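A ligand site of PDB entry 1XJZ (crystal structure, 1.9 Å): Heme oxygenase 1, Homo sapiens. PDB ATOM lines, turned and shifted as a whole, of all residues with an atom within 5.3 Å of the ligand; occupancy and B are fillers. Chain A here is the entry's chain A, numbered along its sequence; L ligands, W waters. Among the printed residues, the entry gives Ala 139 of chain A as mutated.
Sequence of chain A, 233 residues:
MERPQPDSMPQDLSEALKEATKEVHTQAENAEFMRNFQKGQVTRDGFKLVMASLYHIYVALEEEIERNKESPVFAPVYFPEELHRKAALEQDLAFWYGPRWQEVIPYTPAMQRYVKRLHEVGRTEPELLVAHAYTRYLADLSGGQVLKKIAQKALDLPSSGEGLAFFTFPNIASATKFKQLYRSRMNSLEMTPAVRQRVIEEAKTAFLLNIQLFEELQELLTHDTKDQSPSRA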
ATOM      1  N   SER A  14     -17.573  -5.142 -25.136  1.00  0.00           N
ATOM      2  CA  SER A  14     -16.923  -6.430 -24.976  1.00  0.00           C
ATOM      3  C   SER A  14     -16.544  -7.025 -26.327  1.00  0.00           C
ATOM      4  O   SER A  14     -15.466  -7.597 -26.491  1.00  0.00           O
ATOM      5  CB  SER A  14     -17.839  -7.397 -24.221  1.00  0.00           C
ATOM      6  OG  SER A  14     -19.096  -7.507 -24.863  1.00  0.00           O
ATOM      7  N   LEU A  17     -13.709  -4.708 -27.971  1.00  0.00           N
ATOM      8  CA  LEU A  17     -12.393  -4.951 -27.380  1.00  0.00           C
ATOM      9  C   LEU A  17     -11.771  -6.232 -27.932  1.00  0.00           C
ATOM     10  O   LEU A  17     -10.585  -6.270 -28.261  1.00  0.00           O
ATOM     11  CB  LEU A  17     -12.494  -5.071 -25.861  1.00  0.00           C
ATOM     12  CG  LEU A  17     -12.550  -3.755 -25.098  1.00  0.00           C
ATOM     13  CD1 LEU A  17     -12.782  -4.033 -23.642  1.00  0.00           C
ATOM     14  CD2 LEU A  17     -11.260  -2.983 -25.316  1.00  0.00           C
ATOM     15  N   LYS A  18     -12.589  -7.271 -28.010  1.00  0.00           N
ATOM     16  CA  LYS A  18     -12.143  -8.578 -28.494  1.00  0.00           C
ATOM     17  C   LYS A  18     -11.574  -8.496 -29.908  1.00  0.00           C
ATOM     18  O   LYS A  18     -10.487  -9.005 -30.179  1.00  0.00           O
ATOM     19  CB  LYS A  18     -13.307  -9.563 -28.463  1.00  0.00           C
ATOM     20  CG  LYS A  18     -12.921 -10.995 -28.719  1.00  0.00           C
ATOM     21  CD  LYS A  18     -14.150 -11.878 -28.778  1.00  0.00           C
ATOM     22  CE  LYS A  18     -13.764 -13.347 -28.806  1.00  0.00           C
ATOM     23  NZ  LYS A  18     -13.057 -13.716 -27.553  1.00  0.00           N
ATOM     24  N   HIS A  25      -2.956  -9.656 -29.251  1.00  0.00           N
ATOM     25  CA  HIS A  25      -3.100 -10.906 -28.524  1.00  0.00           C
ATOM     26  C   HIS A  25      -2.213 -11.944 -29.205  1.00  0.00           C
ATOM     27  O   HIS A  25      -1.565 -12.743 -28.536  1.00  0.00           O
ATOM     28  CB  HIS A  25      -4.555 -11.366 -28.524  1.00  0.00           C
ATOM     29  CG  HIS A  25      -4.791 -12.620 -27.736  1.00  0.00           C
ATOM     30  ND1 HIS A  25      -4.414 -13.862 -28.186  1.00  0.00           N
ATOM     31  CD2 HIS A  25      -5.328 -12.807 -26.506  1.00  0.00           C
ATOM     32  CE1 HIS A  25      -4.704 -14.762 -27.265  1.00  0.00           C
ATOM     33  NE2 HIS A  25      -5.252 -14.149 -26.235  1.00  0.00           N
ATOM     34  N   ALA A  28       1.126 -11.421 -28.275  1.00  0.00           N
ATOM     35  CA  ALA A  28       1.318 -11.882 -26.902  1.00  0.00           C
ATOM     36  C   ALA A  28       1.636 -13.364 -26.939  1.00  0.00           C
ATOM     37  O   ALA A  28       2.530 -13.842 -26.246  1.00  0.00           O
ATOM     38  CB  ALA A  28       0.059 -11.641 -26.083  1.00  0.00           C
ATOM     39  N   GLU A  29       0.895 -14.104 -27.763  1.00  0.00           N
ATOM     40  CA  GLU A  29       1.103 -15.541 -27.899  1.00  0.00           C
ATOM     41  C   GLU A  29       2.472 -15.851 -28.498  1.00  0.00           C
ATOM     42  O   GLU A  29       3.079 -16.870 -28.175  1.00  0.00           O
ATOM     43  CB  GLU A  29       0.039 -16.144 -28.813  1.00  0.00           C
ATOM     44  CG  GLU A  29      -1.385 -15.847 -28.405  1.00  0.00           C
ATOM     45  CD  GLU A  29      -2.379 -16.333 -29.442  1.00  0.00           C
ATOM     46  OE1 GLU A  29      -2.475 -17.567 -29.652  1.00  0.00           O
ATOM     47  OE2 GLU A  29      -3.057 -15.483 -30.057  1.00  0.00           O
ATOM     48  N   MET A  34       6.218 -16.517 -23.522  1.00  0.00           N
ATOM     49  CA  MET A  34       4.905 -17.139 -23.562  1.00  0.00           C
ATOM     50  C   MET A  34       4.938 -18.340 -24.504  1.00  0.00           C
ATOM     51  O   MET A  34       4.340 -19.370 -24.251  1.00  0.00           O
ATOM     52  CB  MET A  34       3.851 -16.150 -24.060  1.00  0.00           C
ATOM     53  CG  MET A  34       3.154 -15.368 -22.966  1.00  0.00           C
ATOM     54  SD  MET A  34       2.097 -16.390 -21.938  1.00  0.00           S
ATOM     55  CE  MET A  34       3.231 -16.830 -20.637  1.00  0.00           C
ATOM     56  N   GLN A  38       3.946 -21.975 -23.309  1.00  0.00           N
ATOM     57  CA  GLN A  38       2.908 -22.691 -24.034  1.00  0.00           C
ATOM     58  C   GLN A  38       3.390 -24.082 -24.420  1.00  0.00           C
ATOM     59  O   GLN A  38       2.608 -25.035 -24.470  1.00  0.00           O
ATOM     60  CB  GLN A  38       2.506 -21.902 -25.284  1.00  0.00           C
ATOM     61  CG  GLN A  38       1.290 -22.463 -26.009  1.00  0.00           C
ATOM     62  CD  GLN A  38       0.930 -21.652 -27.244  1.00  0.00           C
ATOM     63  OE1 GLN A  38      -0.050 -21.955 -27.932  1.00  0.00           O
ATOM     64  NE2 GLN A  38       1.723 -20.632 -27.536  1.00  0.00           N
ATOM     65  N   TYR A 134     -10.097  -5.632 -17.713  1.00  0.00           N
ATOM     66  CA  TYR A 134     -10.535  -6.583 -18.725  1.00  0.00           C
ATOM     67  C   TYR A 134      -9.369  -7.431 -19.225  1.00  0.00           C
ATOM     68  O   TYR A 134      -9.454  -8.662 -19.280  1.00  0.00           O
ATOM     69  CB  TYR A 134     -11.144  -5.801 -19.901  1.00  0.00           C
ATOM     70  CG  TYR A 134     -11.140  -6.526 -21.222  1.00  0.00           C
ATOM     71  CD1 TYR A 134     -12.137  -7.441 -21.560  1.00  0.00           C
ATOM     72  CD2 TYR A 134     -10.119  -6.304 -22.142  1.00  0.00           C
ATOM     73  CE1 TYR A 134     -12.115  -8.124 -22.776  1.00  0.00           C
ATOM     74  CE2 TYR A 134     -10.081  -6.967 -23.355  1.00  0.00           C
ATOM     75  CZ  TYR A 134     -11.070  -7.879 -23.664  1.00  0.00           C
ATOM     76  OH  TYR A 134     -11.017  -8.511 -24.887  1.00  0.00           O
ATOM     77  N   THR A 135      -8.275  -6.772 -19.576  1.00  0.00           N
ATOM     78  CA  THR A 135      -7.093  -7.453 -20.084  1.00  0.00           C
ATOM     79  C   THR A 135      -6.502  -8.434 -19.074  1.00  0.00           C
ATOM     80  O   THR A 135      -6.226  -9.583 -19.412  1.00  0.00           O
ATOM     81  CB  THR A 135      -6.017  -6.441 -20.493  1.00  0.00           C
ATOM     82  OG1 THR A 135      -6.557  -5.592 -21.520  1.00  0.00           O
ATOM     83  CG2 THR A 135      -4.786  -7.142 -21.024  1.00  0.00           C
ATOM     84  N   ARG A 136      -6.315  -7.980 -17.846  1.00  0.00           N
ATOM     85  CA  ARG A 136      -5.736  -8.831 -16.810  1.00  0.00           C
ATOM     86  C   ARG A 136      -6.652  -9.975 -16.357  1.00  0.00           C
ATOM     87  O   ARG A 136      -6.266 -11.138 -16.431  1.00  0.00           O
ATOM     88  CB  ARG A 136      -5.372  -7.979 -15.601  1.00  0.00           C
ATOM     89  CG  ARG A 136      -3.893  -7.689 -15.467  1.00  0.00           C
ATOM     90  CD  ARG A 136      -3.176  -8.781 -14.681  1.00  0.00           C
ATOM     91  NE  ARG A 136      -3.010 -10.027 -15.435  1.00  0.00           N
ATOM     92  CZ  ARG A 136      -2.143 -10.179 -16.432  1.00  0.00           C
ATOM     93  NH1 ARG A 136      -1.368  -9.167 -16.811  1.00  0.00           N
ATOM     94  NH2 ARG A 136      -2.031 -11.354 -17.043  1.00  0.00           N
ATOM     95  N   LEU A 138      -9.649 -11.194 -17.638  1.00  0.00           N
ATOM     96  CA  LEU A 138     -10.083 -12.142 -18.664  1.00  0.00           C
ATOM     97  C   LEU A 138      -8.910 -12.988 -19.144  1.00  0.00           C
ATOM     98  O   LEU A 138      -9.088 -14.138 -19.542  1.00  0.00           O
ATOM     99  CB  LEU A 138     -10.761 -11.431 -19.839  1.00  0.00           C
ATOM    100  CG  LEU A 138     -12.128 -10.810 -19.518  1.00  0.00           C
ATOM    101  CD1 LEU A 138     -12.954 -10.752 -20.794  1.00  0.00           C
ATOM    102  CD2 LEU A 138     -12.864 -11.641 -18.480  1.00  0.00           C
ATOM    103  N   ALA A 139      -7.706 -12.423 -19.124  1.00  0.00           N
ATOM    104  CA  ALA A 139      -6.531 -13.177 -19.535  1.00  0.00           C
ATOM    105  C   ALA A 139      -6.315 -14.309 -18.524  1.00  0.00           C
ATOM    106  O   ALA A 139      -6.223 -15.476 -18.897  1.00  0.00           O
ATOM    107  CB  ALA A 139      -5.309 -12.274 -19.560  1.00  0.00           C
ATOM    108  N   SER A 142      -9.296 -16.882 -18.562  1.00  0.00           N
ATOM    109  CA  SER A 142      -9.374 -17.720 -19.756  1.00  0.00           C
ATOM    110  C   SER A 142      -8.192 -18.679 -19.906  1.00  0.00           C
ATOM    111  O   SER A 142      -8.375 -19.808 -20.348  1.00  0.00           O
ATOM    112  CB  SER A 142      -9.472 -16.850 -21.008  1.00  0.00           C
ATOM    113  OG  SER A 142     -10.679 -16.106 -21.030  1.00  0.00           O
ATOM    114  N   LYS A 179     -17.745 -14.648 -16.978  1.00  0.00           N
ATOM    115  CA  LYS A 179     -17.303 -13.812 -18.085  1.00  0.00           C
ATOM    116  C   LYS A 179     -18.501 -13.178 -18.792  1.00  0.00           C
ATOM    117  O   LYS A 179     -18.445 -12.035 -19.243  1.00  0.00           O
ATOM    118  CB  LYS A 179     -16.457 -14.642 -19.048  1.00  0.00           C
ATOM    119  CG  LYS A 179     -15.115 -15.063 -18.449  1.00  0.00           C
ATOM    120  CD  LYS A 179     -14.382 -16.112 -19.292  1.00  0.00           C
ATOM    121  CE  LYS A 179     -13.961 -15.566 -20.635  1.00  0.00           C
ATOM    122  NZ  LYS A 179     -13.292 -16.615 -21.458  1.00  0.00           N
ATOM    123  N   ARG A 183     -18.829  -9.245 -19.063  1.00  0.00           N
ATOM    124  CA  ARG A 183     -18.999  -8.559 -20.349  1.00  0.00           C
ATOM    125  C   ARG A 183     -20.227  -7.657 -20.304  1.00  0.00           C
ATOM    126  O   ARG A 183     -20.218  -6.549 -20.831  1.00  0.00           O
ATOM    127  CB  ARG A 183     -19.156  -9.564 -21.483  1.00  0.00           C
ATOM    128  CG  ARG A 183     -17.884 -10.337 -21.794  1.00  0.00           C
ATOM    129  CD  ARG A 183     -17.998 -11.056 -23.132  1.00  0.00           C
ATOM    130  NE  ARG A 183     -16.789 -11.817 -23.435  1.00  0.00           N
ATOM    131  CZ  ARG A 183     -16.604 -13.102 -23.143  1.00  0.00           C
ATOM    132  NH1 ARG A 183     -17.568 -13.798 -22.541  1.00  0.00           N
ATOM    133  NH2 ARG A 183     -15.451 -13.689 -23.444  1.00  0.00           N
ATOM    134  N   PHE A 207      -1.894  -4.966 -23.362  1.00  0.00           N
ATOM    135  CA  PHE A 207      -1.255  -6.136 -23.967  1.00  0.00           C
ATOM    136  C   PHE A 207       0.220  -5.854 -24.191  1.00  0.00           C
ATOM    137  O   PHE A 207       1.077  -6.662 -23.860  1.00  0.00           O
ATOM    138  CB  PHE A 207      -1.896  -6.499 -25.312  1.00  0.00           C
ATOM    139  CG  PHE A 207      -3.079  -7.394 -25.204  1.00  0.00           C
ATOM    140  CD1 PHE A 207      -4.353  -6.869 -24.994  1.00  0.00           C
ATOM    141  CD2 PHE A 207      -2.924  -8.769 -25.301  1.00  0.00           C
ATOM    142  CE1 PHE A 207      -5.448  -7.706 -24.890  1.00  0.00           C
ATOM    143  CE2 PHE A 207      -4.015  -9.615 -25.198  1.00  0.00           C
ATOM    144  CZ  PHE A 207      -5.281  -9.086 -24.991  1.00  0.00           C
ATOM    145  N   ASN A 210       2.350  -6.222 -21.243  1.00  0.00           N
ATOM    146  CA  ASN A 210       2.560  -7.619 -20.920  1.00  0.00           C
ATOM    147  C   ASN A 210       3.616  -8.191 -21.849  1.00  0.00           C
ATOM    148  O   ASN A 210       4.480  -8.963 -21.421  1.00  0.00           O
ATOM    149  CB  ASN A 210       1.257  -8.392 -21.079  1.00  0.00           C
ATOM    150  CG  ASN A 210       0.388  -8.301 -19.862  1.00  0.00           C
ATOM    151  OD1 ASN A 210       0.601  -9.028 -18.889  1.00  0.00           O
ATOM    152  ND2 ASN A 210      -0.577  -7.397 -19.877  1.00  0.00           N
ATOM    153  N   PHE A 214       7.249  -9.842 -20.920  1.00  0.00           N
ATOM    154  CA  PHE A 214       7.703 -11.156 -21.394  1.00  0.00           C
ATOM    155  C   PHE A 214       9.095 -11.048 -21.978  1.00  0.00           C
ATOM    156  O   PHE A 214       9.985 -11.816 -21.632  1.00  0.00           O
ATOM    157  CB  PHE A 214       6.771 -11.721 -22.470  1.00  0.00           C
ATOM    158  CG  PHE A 214       5.373 -11.988 -21.998  1.00  0.00           C
ATOM    159  CD1 PHE A 214       5.127 -12.373 -20.691  1.00  0.00           C
ATOM    160  CD2 PHE A 214       4.302 -11.884 -22.887  1.00  0.00           C
ATOM    161  CE1 PHE A 214       3.833 -12.642 -20.262  1.00  0.00           C
ATOM    162  CE2 PHE A 214       3.004 -12.154 -22.467  1.00  0.00           C
ATOM    163  CZ  PHE A 214       2.773 -12.532 -21.145  1.00  0.00           C
HETATM  164  C1  LIG L   1      -8.860 -15.077 -24.495  1.00  0.00           C
HETATM  165  C2  LIG L   1      -5.336 -18.119 -25.936  1.00  0.00           C
HETATM  166  C3  LIG L   1      -2.015 -15.213 -23.981  1.00  0.00           C
HETATM  167  C4  LIG L   1      -5.477 -11.988 -22.871  1.00  0.00           C
HETATM  168  C5  LIG L   1      -8.173 -16.189 -25.018  1.00  0.00           C
HETATM  169  C6  LIG L   1      -8.811 -17.317 -25.678  1.00  0.00           C
HETATM  170  C7  LIG L   1      -7.808 -18.139 -26.131  1.00  0.00           C
HETATM  171  C8  LIG L   1      -6.559 -17.510 -25.754  1.00  0.00           C
HETATM  172  C9  LIG L   1      -7.979 -19.497 -26.796  1.00  0.00           C
HETATM  173  C10 LIG L   1     -10.297 -17.612 -25.746  1.00  0.00           C
HETATM  174  C11 LIG L   1     -11.017 -16.957 -26.921  1.00  0.00           C
HETATM  175  C12 LIG L   1     -12.494 -17.316 -26.960  1.00  0.00           C
HETATM  176  O1  LIG L   1     -12.822 -18.515 -27.040  1.00  0.00           O
HETATM  177  O2  LIG L   1     -13.331 -16.389 -26.892  1.00  0.00           O
HETATM  178  C13 LIG L   1      -4.137 -17.619 -25.462  1.00  0.00           C
HETATM  179  C14 LIG L   1      -2.877 -18.311 -25.569  1.00  0.00           C
HETATM  180  C15 LIG L   1      -1.925 -17.490 -25.045  1.00  0.00           C
HETATM  181  C16 LIG L   1      -2.629 -16.285 -24.594  1.00  0.00           C
HETATM  182  C17 LIG L   1      -2.687 -19.728 -26.157  1.00  0.00           C
HETATM  183  C18 LIG L   1      -0.540 -17.701 -24.913  1.00  0.00           C
HETATM  184  C19 LIG L   1       0.319 -18.640 -25.652  1.00  0.00           C
HETATM  185  C20 LIG L   1      -2.677 -14.088 -23.499  1.00  0.00           C
HETATM  186  C21 LIG L   1      -2.005 -12.964 -22.880  1.00  0.00           C
HETATM  187  C22 LIG L   1      -2.959 -12.035 -22.585  1.00  0.00           C
HETATM  188  C23 LIG L   1      -4.240 -12.624 -22.990  1.00  0.00           C
HETATM  189  C24 LIG L   1      -0.522 -12.911 -22.564  1.00  0.00           C
HETATM  190  C25 LIG L   1      -2.782 -10.751 -22.069  1.00  0.00           C
HETATM  191  C26 LIG L   1      -1.782 -10.386 -21.059  1.00  0.00           C
HETATM  192  C27 LIG L   1      -6.701 -12.536 -23.257  1.00  0.00           C
HETATM  193  C28 LIG L   1      -7.968 -11.883 -23.067  1.00  0.00           C
HETATM  194  C29 LIG L   1      -8.920 -12.750 -23.500  1.00  0.00           C
HETATM  195  C30 LIG L   1      -8.231 -13.940 -23.970  1.00  0.00           C
HETATM  196  C31 LIG L   1      -8.213 -10.483 -22.523  1.00  0.00           C
HETATM  197  C32 LIG L   1     -10.422 -12.455 -23.513  1.00  0.00           C
HETATM  198  C33 LIG L   1     -10.960 -12.199 -24.917  1.00  0.00           C
HETATM  199  C34 LIG L   1     -12.395 -11.699 -24.907  1.00  0.00           C
HETATM  200  O3  LIG L   1     -12.599 -10.472 -25.016  1.00  0.00           O
HETATM  201  O4  LIG L   1     -13.310 -12.533 -24.765  1.00  0.00           O
HETATM  202  N1  LIG L   1      -6.780 -16.303 -25.072  1.00  0.00           N
HETATM  203  N2  LIG L   1      -4.000 -16.381 -24.832  1.00  0.00           N
HETATM  204  N3  LIG L   1      -4.056 -13.886 -23.567  1.00  0.00           N
HETATM  205  N4  LIG L   1      -6.855 -13.795 -23.836  1.00  0.00           N
HETATM  206 FE1  LIG L   1      -5.440 -15.066 -24.338  1.00  0.00          FE
HETATM  207  O   HOH W   1     -12.811 -15.077 -23.695  1.00  0.00           O
HETATM  208  O   HOH W   2      -5.715 -15.915 -22.478  1.00  0.00           O
HETATM  209  O   HOH W   3      -4.868 -19.340 -22.887  1.00  0.00           O
HETATM  210  O   HOH W   4      -1.015 -19.662 -22.191  1.00  0.00           O
HETATM  211  O   HOH W   5     -15.390  -9.885 -24.895  1.00  0.00           O
HETATM  212  O   HOH W   6      -8.637  -9.454 -25.536  1.00  0.00           O
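OE2 of Glu 29 lies within hydrogen-bond range of ND1 of His 25 (2.8 Å). OD1 of Asn 210 sits at hydrogen-bond distance from NH1 of Arg 136 (2.9 Å). O of Leu 138 sits at hydrogen-bond distance from OG of Ser 142, at 2.9 Å. NZ of Lys 179 sits at hydrogen-bond distance from OG of Ser 142 (2.7 Å).
NE2 of His 25 binds FE1 of the ligand (2.1 Å). The side-chain hydroxyl (OH) of Tyr 134 is in hydrogen-bond range of an oxygen (O3) of the ligand (2.5 Å). O2 of the ligand lies within salt-bridge range of NZ of Lys 18 (2.8 Å). The guanidinium group of Arg 183 is in salt-bridge range of an oxygen (O4) of the ligand.
Ala 28 touches the ligand. Glu 29 touches the ligand (CG to C15, 3.8 Å). NE2 of Gln 38 touches C19 of the ligand, 3.1 Å away. O of Thr 135 touches C31 of the ligand, 3.8 Å away. Leu 138 touches the ligand. Ala 139 touches the ligand. CB of Ser 142 touches C1 of the ligand, at 3.96 Å. Phe 207 touches the ligand (CE2 to C25, 3.5 Å). Asn 210 touches the ligand (CG to C26, 3.2 Å). CZ of Phe 214 touches C24 of the ligand, at 3.6 Å. Hydrophobic or aromatic side chains within 4 Å of the ligand: His 25, Ala 28, Tyr 134, Leu 138, Ala 139, Phe 207 and Phe 214.
Water W1 lies within hydrogen-bond range of the side-chain amino group (NZ) of Lys 179 (2.8 Å), an oxygen (O4) of the ligand (2.8 Å) and the guanidinium group (NH2) of Arg 183 (3.0 Å). Water W5 lies within hydrogen-bond range of the backbone carbonyl oxygen (O) of Ser 14 (2.8 Å), the guanidinium group (NE) of Arg 183 (2.8 Å) and an oxygen (O3) of the ligand (2.9 Å).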
